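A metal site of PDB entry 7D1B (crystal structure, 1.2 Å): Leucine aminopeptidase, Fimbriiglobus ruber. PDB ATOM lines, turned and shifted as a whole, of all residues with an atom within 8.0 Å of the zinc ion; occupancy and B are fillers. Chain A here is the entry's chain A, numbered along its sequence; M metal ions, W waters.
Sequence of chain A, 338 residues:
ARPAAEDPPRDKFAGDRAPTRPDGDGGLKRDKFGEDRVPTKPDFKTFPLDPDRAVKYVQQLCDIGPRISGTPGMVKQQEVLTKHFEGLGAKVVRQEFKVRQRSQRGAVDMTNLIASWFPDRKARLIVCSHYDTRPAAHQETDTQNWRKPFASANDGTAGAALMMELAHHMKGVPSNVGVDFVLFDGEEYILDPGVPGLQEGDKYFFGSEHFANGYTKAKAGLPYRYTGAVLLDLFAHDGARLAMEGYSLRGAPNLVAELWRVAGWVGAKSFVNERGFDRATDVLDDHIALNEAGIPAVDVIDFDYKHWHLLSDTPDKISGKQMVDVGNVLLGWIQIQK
Water W1 bridges the indole nitrogen (NE1) of Trp 308 (3.1 Å) and the side-chain carboxylate (OD1) of Asp 155 (3.5 Å).
The zinc ion is bound by the side-chain carboxylate of Glu 188 (2.0 Å), the side-chain carboxylate of Asp 155 (2.0 Å), a ring nitrogen (NE2) of His 309 (2.0 Å) and water W1 (2.1 Å).
Slightly farther from the zinc ion lies the side-chain carboxylate (OE1) of Glu 188 (2.8 Å).
Residues that only touch the zinc ion: Trp 308 (3.98 Å).
Four residues have an atom within 4 Å of the zinc ion: Asp 155, Glu 188, Trp 308 and His 309.
Along chain A the residues within 4 Å of the zinc ion span positions 155 to 309.
The nearest printed residue that does not touch the zinc ion is Glu 187 (4.7 Å).
The guanidinium group (NH2) of Arg 134 lies within salt-bridge range of the side-chain carboxylate (OE1) of Glu 188, at 2.9 Å.
The backbone NH (N) of Glu 188 sits at hydrogen-bond distance from the side-chain carboxylate (OD2) of Asp 132 (3.0 Å).
The side-chain carboxylate (OD1) of Asp 155 is in hydrogen-bond range of a ring nitrogen (NE2) of His 130, 2.7 Å away.
OG of Ser 152 sits at hydrogen-bond distance from O of Asp 155.
NE2 of His 309 sits close to NE1 of Trp 308, at 3.4 Å.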
ATOM      1  N   HIS A 130      19.943  15.323 -19.256  1.00  0.00           N
ATOM      2  CA  HIS A 130      21.074  14.973 -18.390  1.00  0.00           C
ATOM      3  C   HIS A 130      20.571  14.795 -16.960  1.00  0.00           C
ATOM      4  O   HIS A 130      19.458  15.222 -16.616  1.00  0.00           O
ATOM      5  CB  HIS A 130      22.257  15.948 -18.515  1.00  0.00           C
ATOM      6  CG  HIS A 130      22.161  17.190 -17.667  1.00  0.00           C
ATOM      7  ND1 HIS A 130      22.989  17.406 -16.586  1.00  0.00           N
ATOM      8  CD2 HIS A 130      21.425  18.320 -17.805  1.00  0.00           C
ATOM      9  CE1 HIS A 130      22.737  18.603 -16.077  1.00  0.00           C
ATOM     10  NE2 HIS A 130      21.787  19.169 -16.795  1.00  0.00           N
ATOM     11  N   ASP A 132      23.384  14.394 -14.254  1.00  0.00           N
ATOM     12  CA  ASP A 132      24.435  14.890 -13.368  1.00  0.00           C
ATOM     13  C   ASP A 132      24.158  16.347 -13.047  1.00  0.00           C
ATOM     14  O   ASP A 132      23.512  17.059 -13.809  1.00  0.00           O
ATOM     15  CB  ASP A 132      25.812  14.729 -14.021  1.00  0.00           C
ATOM     16  CG  ASP A 132      25.980  15.612 -15.246  1.00  0.00           C
ATOM     17  OD1 ASP A 132      25.116  15.573 -16.164  1.00  0.00           O
ATOM     18  OD2 ASP A 132      27.010  16.324 -15.334  1.00  0.00           O
ATOM     19  N   THR A 133      24.647  16.808 -11.907  1.00  0.00           N
ATOM     20  CA  THR A 133      24.527  18.223 -11.565  1.00  0.00           C
ATOM     21  C   THR A 133      25.886  18.875 -11.622  1.00  0.00           C
ATOM     22  O   THR A 133      26.907  18.276 -11.253  1.00  0.00           O
ATOM     23  CB  THR A 133      23.820  18.467 -10.226  1.00  0.00           C
ATOM     24  OG1 THR A 133      24.551  17.864  -9.148  1.00  0.00           O
ATOM     25  CG2 THR A 133      22.388  17.911 -10.250  1.00  0.00           C
ATOM     26  N   ARG A 134      25.921  20.119 -12.083  1.00  0.00           N
ATOM     27  CA  ARG A 134      27.165  20.839 -12.226  1.00  0.00           C
ATOM     28  C   ARG A 134      27.826  21.006 -10.855  1.00  0.00           C
ATOM     29  O   ARG A 134      27.137  21.254  -9.863  1.00  0.00           O
ATOM     30  CB  ARG A 134      26.870  22.214 -12.810  1.00  0.00           C
ATOM     31  CG  ARG A 134      28.076  22.909 -13.393  1.00  0.00           C
ATOM     32  CD  ARG A 134      27.671  24.265 -13.969  1.00  0.00           C
ATOM     33  NE  ARG A 134      28.828  24.977 -14.487  1.00  0.00           N
ATOM     34  CZ  ARG A 134      29.220  25.004 -15.759  1.00  0.00           C
ATOM     35  NH1 ARG A 134      30.334  25.672 -16.073  1.00  0.00           N
ATOM     36  NH2 ARG A 134      28.551  24.345 -16.697  1.00  0.00           N
ATOM     37  N   ALA A 136      29.406  23.372  -9.432  1.00  0.00           N
ATOM     38  CA  ALA A 136      29.258  24.677  -8.811  1.00  0.00           C
ATOM     39  C   ALA A 136      28.313  25.527  -9.642  1.00  0.00           C
ATOM     40  O   ALA A 136      28.188  25.338 -10.856  1.00  0.00           O
ATOM     41  CB  ALA A 136      30.598  25.404  -8.671  1.00  0.00           C
ATOM     42  N   PHE A 150      24.879  23.082  -5.276  1.00  0.00           N
ATOM     43  CA  PHE A 150      24.077  23.581  -6.382  1.00  0.00           C
ATOM     44  C   PHE A 150      22.992  22.549  -6.705  1.00  0.00           C
ATOM     45  O   PHE A 150      23.296  21.433  -7.158  1.00  0.00           O
ATOM     46  CB  PHE A 150      24.979  23.866  -7.581  1.00  0.00           C
ATOM     47  CG  PHE A 150      24.232  24.210  -8.849  1.00  0.00           C
ATOM     48  CD1 PHE A 150      23.289  25.238  -8.878  1.00  0.00           C
ATOM     49  CD2 PHE A 150      24.477  23.498 -10.001  1.00  0.00           C
ATOM     50  CE1 PHE A 150      22.596  25.531 -10.069  1.00  0.00           C
ATOM     51  CE2 PHE A 150      23.799  23.796 -11.195  1.00  0.00           C
ATOM     52  CZ  PHE A 150      22.837  24.811 -11.215  1.00  0.00           C
ATOM     53  N   SER A 152      20.429  22.672  -8.945  1.00  0.00           N
ATOM     54  CA  SER A 152      20.204  22.427 -10.371  1.00  0.00           C
ATOM     55  C   SER A 152      18.767  21.971 -10.669  1.00  0.00           C
ATOM     56  O   SER A 152      18.559  21.087 -11.487  1.00  0.00           O
ATOM     57  CB  SER A 152      21.225  21.395 -10.883  1.00  0.00           C
ATOM     58  OG  SER A 152      21.336  21.410 -12.281  1.00  0.00           O
ATOM     59  N   ASN A 154      16.083  23.080 -12.300  1.00  0.00           N
ATOM     60  CA  ASN A 154      15.551  23.184 -13.660  1.00  0.00           C
ATOM     61  C   ASN A 154      16.534  22.700 -14.704  1.00  0.00           C
ATOM     62  O   ASN A 154      16.324  22.925 -15.899  1.00  0.00           O
ATOM     63  CB  ASN A 154      15.158  24.637 -13.936  1.00  0.00           C
ATOM     64  CG  ASN A 154      14.248  24.800 -15.154  1.00  0.00           C
ATOM     65  OD1 ASN A 154      13.409  23.937 -15.453  1.00  0.00           O
ATOM     66  ND2 ASN A 154      14.406  25.928 -15.843  1.00  0.00           N
ATOM     67  N   ASP A 155      17.618  22.053 -14.298  1.00  0.00           N
ATOM     68  CA  ASP A 155      18.760  21.811 -15.173  1.00  0.00           C
ATOM     69  C   ASP A 155      19.132  20.347 -15.002  1.00  0.00           C
ATOM     70  O   ASP A 155      19.839  19.969 -14.054  1.00  0.00           O
ATOM     71  CB  ASP A 155      19.845  22.799 -14.755  1.00  0.00           C
ATOM     72  CG  ASP A 155      21.077  22.760 -15.638  1.00  0.00           C
ATOM     73  OD1 ASP A 155      21.234  21.836 -16.466  1.00  0.00           O
ATOM     74  OD2 ASP A 155      21.936  23.680 -15.472  1.00  0.00           O
ATOM     75  N   GLY A 156      18.597  19.503 -15.872  1.00  0.00           N
ATOM     76  CA  GLY A 156      18.673  18.062 -15.745  1.00  0.00           C
ATOM     77  C   GLY A 156      17.622  17.506 -14.811  1.00  0.00           C
ATOM     78  O   GLY A 156      16.817  16.659 -15.205  1.00  0.00           O
ATOM     79  N   GLU A 187      27.034  15.478 -18.429  1.00  0.00           N
ATOM     80  CA  GLU A 187      26.837  16.600 -19.339  1.00  0.00           C
ATOM     81  C   GLU A 187      27.706  17.784 -18.949  1.00  0.00           C
ATOM     82  O   GLU A 187      28.260  18.468 -19.812  1.00  0.00           O
ATOM     83  CB  GLU A 187      25.377  17.048 -19.408  1.00  0.00           C
ATOM     84  CG  GLU A 187      25.149  18.089 -20.494  1.00  0.00           C
ATOM     85  CD  GLU A 187      24.746  19.413 -19.967  1.00  0.00           C
ATOM     86  OE1 GLU A 187      24.170  19.491 -18.866  1.00  0.00           O
ATOM     87  OE2 GLU A 187      25.037  20.393 -20.676  1.00  0.00           O
ATOM     88  N   GLU A 188      27.812  18.065 -17.648  1.00  0.00           N
ATOM     89  CA  GLU A 188      28.529  19.253 -17.209  1.00  0.00           C
ATOM     90  C   GLU A 188      29.225  18.994 -15.879  1.00  0.00           C
ATOM     91  O   GLU A 188      29.017  19.685 -14.865  1.00  0.00           O
ATOM     92  CB  GLU A 188      27.638  20.495 -17.233  1.00  0.00           C
ATOM     93  CG  GLU A 188      26.381  20.440 -16.411  1.00  0.00           C
ATOM     94  CD  GLU A 188      25.601  21.737 -16.547  1.00  0.00           C
ATOM     95  OE1 GLU A 188      26.169  22.737 -17.072  1.00  0.00           O
ATOM     96  OE2 GLU A 188      24.398  21.780 -16.152  1.00  0.00           O
ATOM     97  N   ILE A 190      31.837  19.973 -14.606  1.00  0.00           N
ATOM     98  CA  ILE A 190      32.770  21.078 -14.853  1.00  0.00           C
ATOM     99  C   ILE A 190      33.427  21.456 -13.524  1.00  0.00           C
ATOM    100  O   ILE A 190      32.835  22.145 -12.690  1.00  0.00           O
ATOM    101  CB  ILE A 190      32.079  22.274 -15.494  1.00  0.00           C
ATOM    102  CG1 ILE A 190      31.323  21.873 -16.765  1.00  0.00           C
ATOM    103  CG2 ILE A 190      33.108  23.391 -15.763  1.00  0.00           C
ATOM    104  CD1 ILE A 190      32.142  21.111 -17.827  1.00  0.00           C
ATOM    105  N   TYR A 204      32.238  19.079 -21.877  1.00  0.00           N
ATOM    106  CA  TYR A 204      30.816  18.781 -21.748  1.00  0.00           C
ATOM    107  C   TYR A 204      30.461  17.516 -22.521  1.00  0.00           C
ATOM    108  O   TYR A 204      31.175  17.074 -23.426  1.00  0.00           O
ATOM    109  CB  TYR A 204      30.000  19.939 -22.329  1.00  0.00           C
ATOM    110  CG  TYR A 204      30.003  21.202 -21.509  1.00  0.00           C
ATOM    111  CD1 TYR A 204      31.122  22.031 -21.448  1.00  0.00           C
ATOM    112  CD2 TYR A 204      28.848  21.591 -20.838  1.00  0.00           C
ATOM    113  CE1 TYR A 204      31.089  23.208 -20.698  1.00  0.00           C
ATOM    114  CE2 TYR A 204      28.814  22.752 -20.093  1.00  0.00           C
ATOM    115  CZ  TYR A 204      29.928  23.558 -20.029  1.00  0.00           C
ATOM    116  OH  TYR A 204      29.833  24.714 -19.285  1.00  0.00           O
ATOM    117  N   ASP A 233      15.698  20.441 -21.397  1.00  0.00           N
ATOM    118  CA  ASP A 233      16.720  21.148 -20.630  1.00  0.00           C
ATOM    119  C   ASP A 233      16.219  22.564 -20.331  1.00  0.00           C
ATOM    120  O   ASP A 233      15.810  23.264 -21.259  1.00  0.00           O
ATOM    121  CB  ASP A 233      18.001  21.240 -21.463  1.00  0.00           C
ATOM    122  CG  ASP A 233      19.248  21.527 -20.624  1.00  0.00           C
ATOM    123  OD1 ASP A 233      19.151  21.604 -19.369  1.00  0.00           O
ATOM    124  OD2 ASP A 233      20.368  21.672 -21.207  1.00  0.00           O
ATOM    125  N   LEU A 234      16.247  22.999 -19.076  1.00  0.00           N
ATOM    126  CA  LEU A 234      15.866  24.374 -18.722  1.00  0.00           C
ATOM    127  C   LEU A 234      14.474  24.718 -19.276  1.00  0.00           C
ATOM    128  O   LEU A 234      14.289  25.737 -19.946  1.00  0.00           O
ATOM    129  CB  LEU A 234      16.898  25.411 -19.184  1.00  0.00           C
ATOM    130  CG  LEU A 234      18.363  25.119 -18.893  1.00  0.00           C
ATOM    131  CD1 LEU A 234      19.207  26.225 -19.506  1.00  0.00           C
ATOM    132  CD2 LEU A 234      18.632  25.016 -17.425  1.00  0.00           C
ATOM    133  N   ASP A 285      24.364  21.306 -26.657  1.00  0.00           N
ATOM    134  CA  ASP A 285      23.692  20.558 -25.600  1.00  0.00           C
ATOM    135  C   ASP A 285      23.807  19.073 -25.947  1.00  0.00           C
ATOM    136  O   ASP A 285      24.469  18.670 -26.911  1.00  0.00           O
ATOM    137  CB  ASP A 285      22.254  21.052 -25.455  1.00  0.00           C
ATOM    138  CG  ASP A 285      21.726  20.945 -24.050  1.00  0.00           C
ATOM    139  OD1 ASP A 285      22.287  20.208 -23.226  1.00  0.00           O
ATOM    140  OD2 ASP A 285      20.685  21.603 -23.769  1.00  0.00           O
ATOM    141  N   PHE A 303      16.785  29.011 -22.945  1.00  0.00           N
ATOM    142  CA  PHE A 303      18.134  29.287 -22.481  1.00  0.00           C
ATOM    143  C   PHE A 303      18.229  30.618 -21.749  1.00  0.00           C
ATOM    144  O   PHE A 303      19.288  30.922 -21.221  1.00  0.00           O
ATOM    145  CB  PHE A 303      19.100  29.201 -23.673  1.00  0.00           C
ATOM    146  CG  PHE A 303      20.561  29.027 -23.307  1.00  0.00           C
ATOM    147  CD1 PHE A 303      20.987  28.334 -22.167  1.00  0.00           C
ATOM    148  CD2 PHE A 303      21.534  29.577 -24.139  1.00  0.00           C
ATOM    149  CE1 PHE A 303      22.355  28.198 -21.880  1.00  0.00           C
ATOM    150  CE2 PHE A 303      22.892  29.439 -23.841  1.00  0.00           C
ATOM    151  CZ  PHE A 303      23.292  28.742 -22.719  1.00  0.00           C
ATOM    152  N   TRP A 308      19.734  30.205 -14.211  1.00  0.00           N
ATOM    153  CA  TRP A 308      20.716  29.296 -14.804  1.00  0.00           C
ATOM    154  C   TRP A 308      22.060  29.389 -14.089  1.00  0.00           C
ATOM    155  O   TRP A 308      22.667  30.467 -14.013  1.00  0.00           O
ATOM    156  CB  TRP A 308      20.874  29.695 -16.258  1.00  0.00           C
ATOM    157  CG  TRP A 308      21.852  28.858 -17.026  1.00  0.00           C
ATOM    158  CD1 TRP A 308      21.791  27.516 -17.267  1.00  0.00           C
ATOM    159  CD2 TRP A 308      23.030  29.332 -17.692  1.00  0.00           C
ATOM    160  NE1 TRP A 308      22.853  27.129 -18.043  1.00  0.00           N
ATOM    161  CE2 TRP A 308      23.623  28.226 -18.325  1.00  0.00           C
ATOM    162  CE3 TRP A 308      23.624  30.594 -17.823  1.00  0.00           C
ATOM    163  CZ2 TRP A 308      24.812  28.334 -19.067  1.00  0.00           C
ATOM    164  CZ3 TRP A 308      24.802  30.701 -18.555  1.00  0.00           C
ATOM    165  CH2 TRP A 308      25.367  29.581 -19.170  1.00  0.00           C
ATOM    166  N   HIS A 309      22.507  28.251 -13.556  1.00  0.00           N
ATOM    167  CA  HIS A 309      23.797  28.152 -12.885  1.00  0.00           C
ATOM    168  C   HIS A 309      23.929  29.129 -11.714  1.00  0.00           C
ATOM    169  O   HIS A 309      25.036  29.565 -11.380  1.00  0.00           O
ATOM    170  CB  HIS A 309      24.952  28.225 -13.880  1.00  0.00           C
ATOM    171  CG  HIS A 309      24.955  27.069 -14.830  1.00  0.00           C
ATOM    172  ND1 HIS A 309      25.808  26.959 -15.907  1.00  0.00           N
ATOM    173  CD2 HIS A 309      24.198  25.938 -14.844  1.00  0.00           C
ATOM    174  CE1 HIS A 309      25.534  25.840 -16.565  1.00  0.00           C
ATOM    175  NE2 HIS A 309      24.586  25.182 -15.918  1.00  0.00           N
ATOM    176  N   ASP A 313      18.560  28.193  -8.446  1.00  0.00           N
ATOM    177  CA  ASP A 313      17.918  27.188  -9.299  1.00  0.00           C
ATOM    178  C   ASP A 313      17.438  26.039  -8.423  1.00  0.00           C
ATOM    179  O   ASP A 313      18.077  24.994  -8.310  1.00  0.00           O
ATOM    180  CB  ASP A 313      18.891  26.716 -10.382  1.00  0.00           C
ATOM    181  CG  ASP A 313      18.280  25.711 -11.335  1.00  0.00           C
ATOM    182  OD1 ASP A 313      17.034  25.573 -11.358  1.00  0.00           O
ATOM    183  OD2 ASP A 313      19.053  25.046 -12.072  1.00  0.00           O
HETATM  184 ZN    ZN M   1      23.585  23.523 -16.517  1.00  0.00          ZN
HETATM  185  O   HOH W   1      22.972  24.093 -18.445  1.00  0.00           O
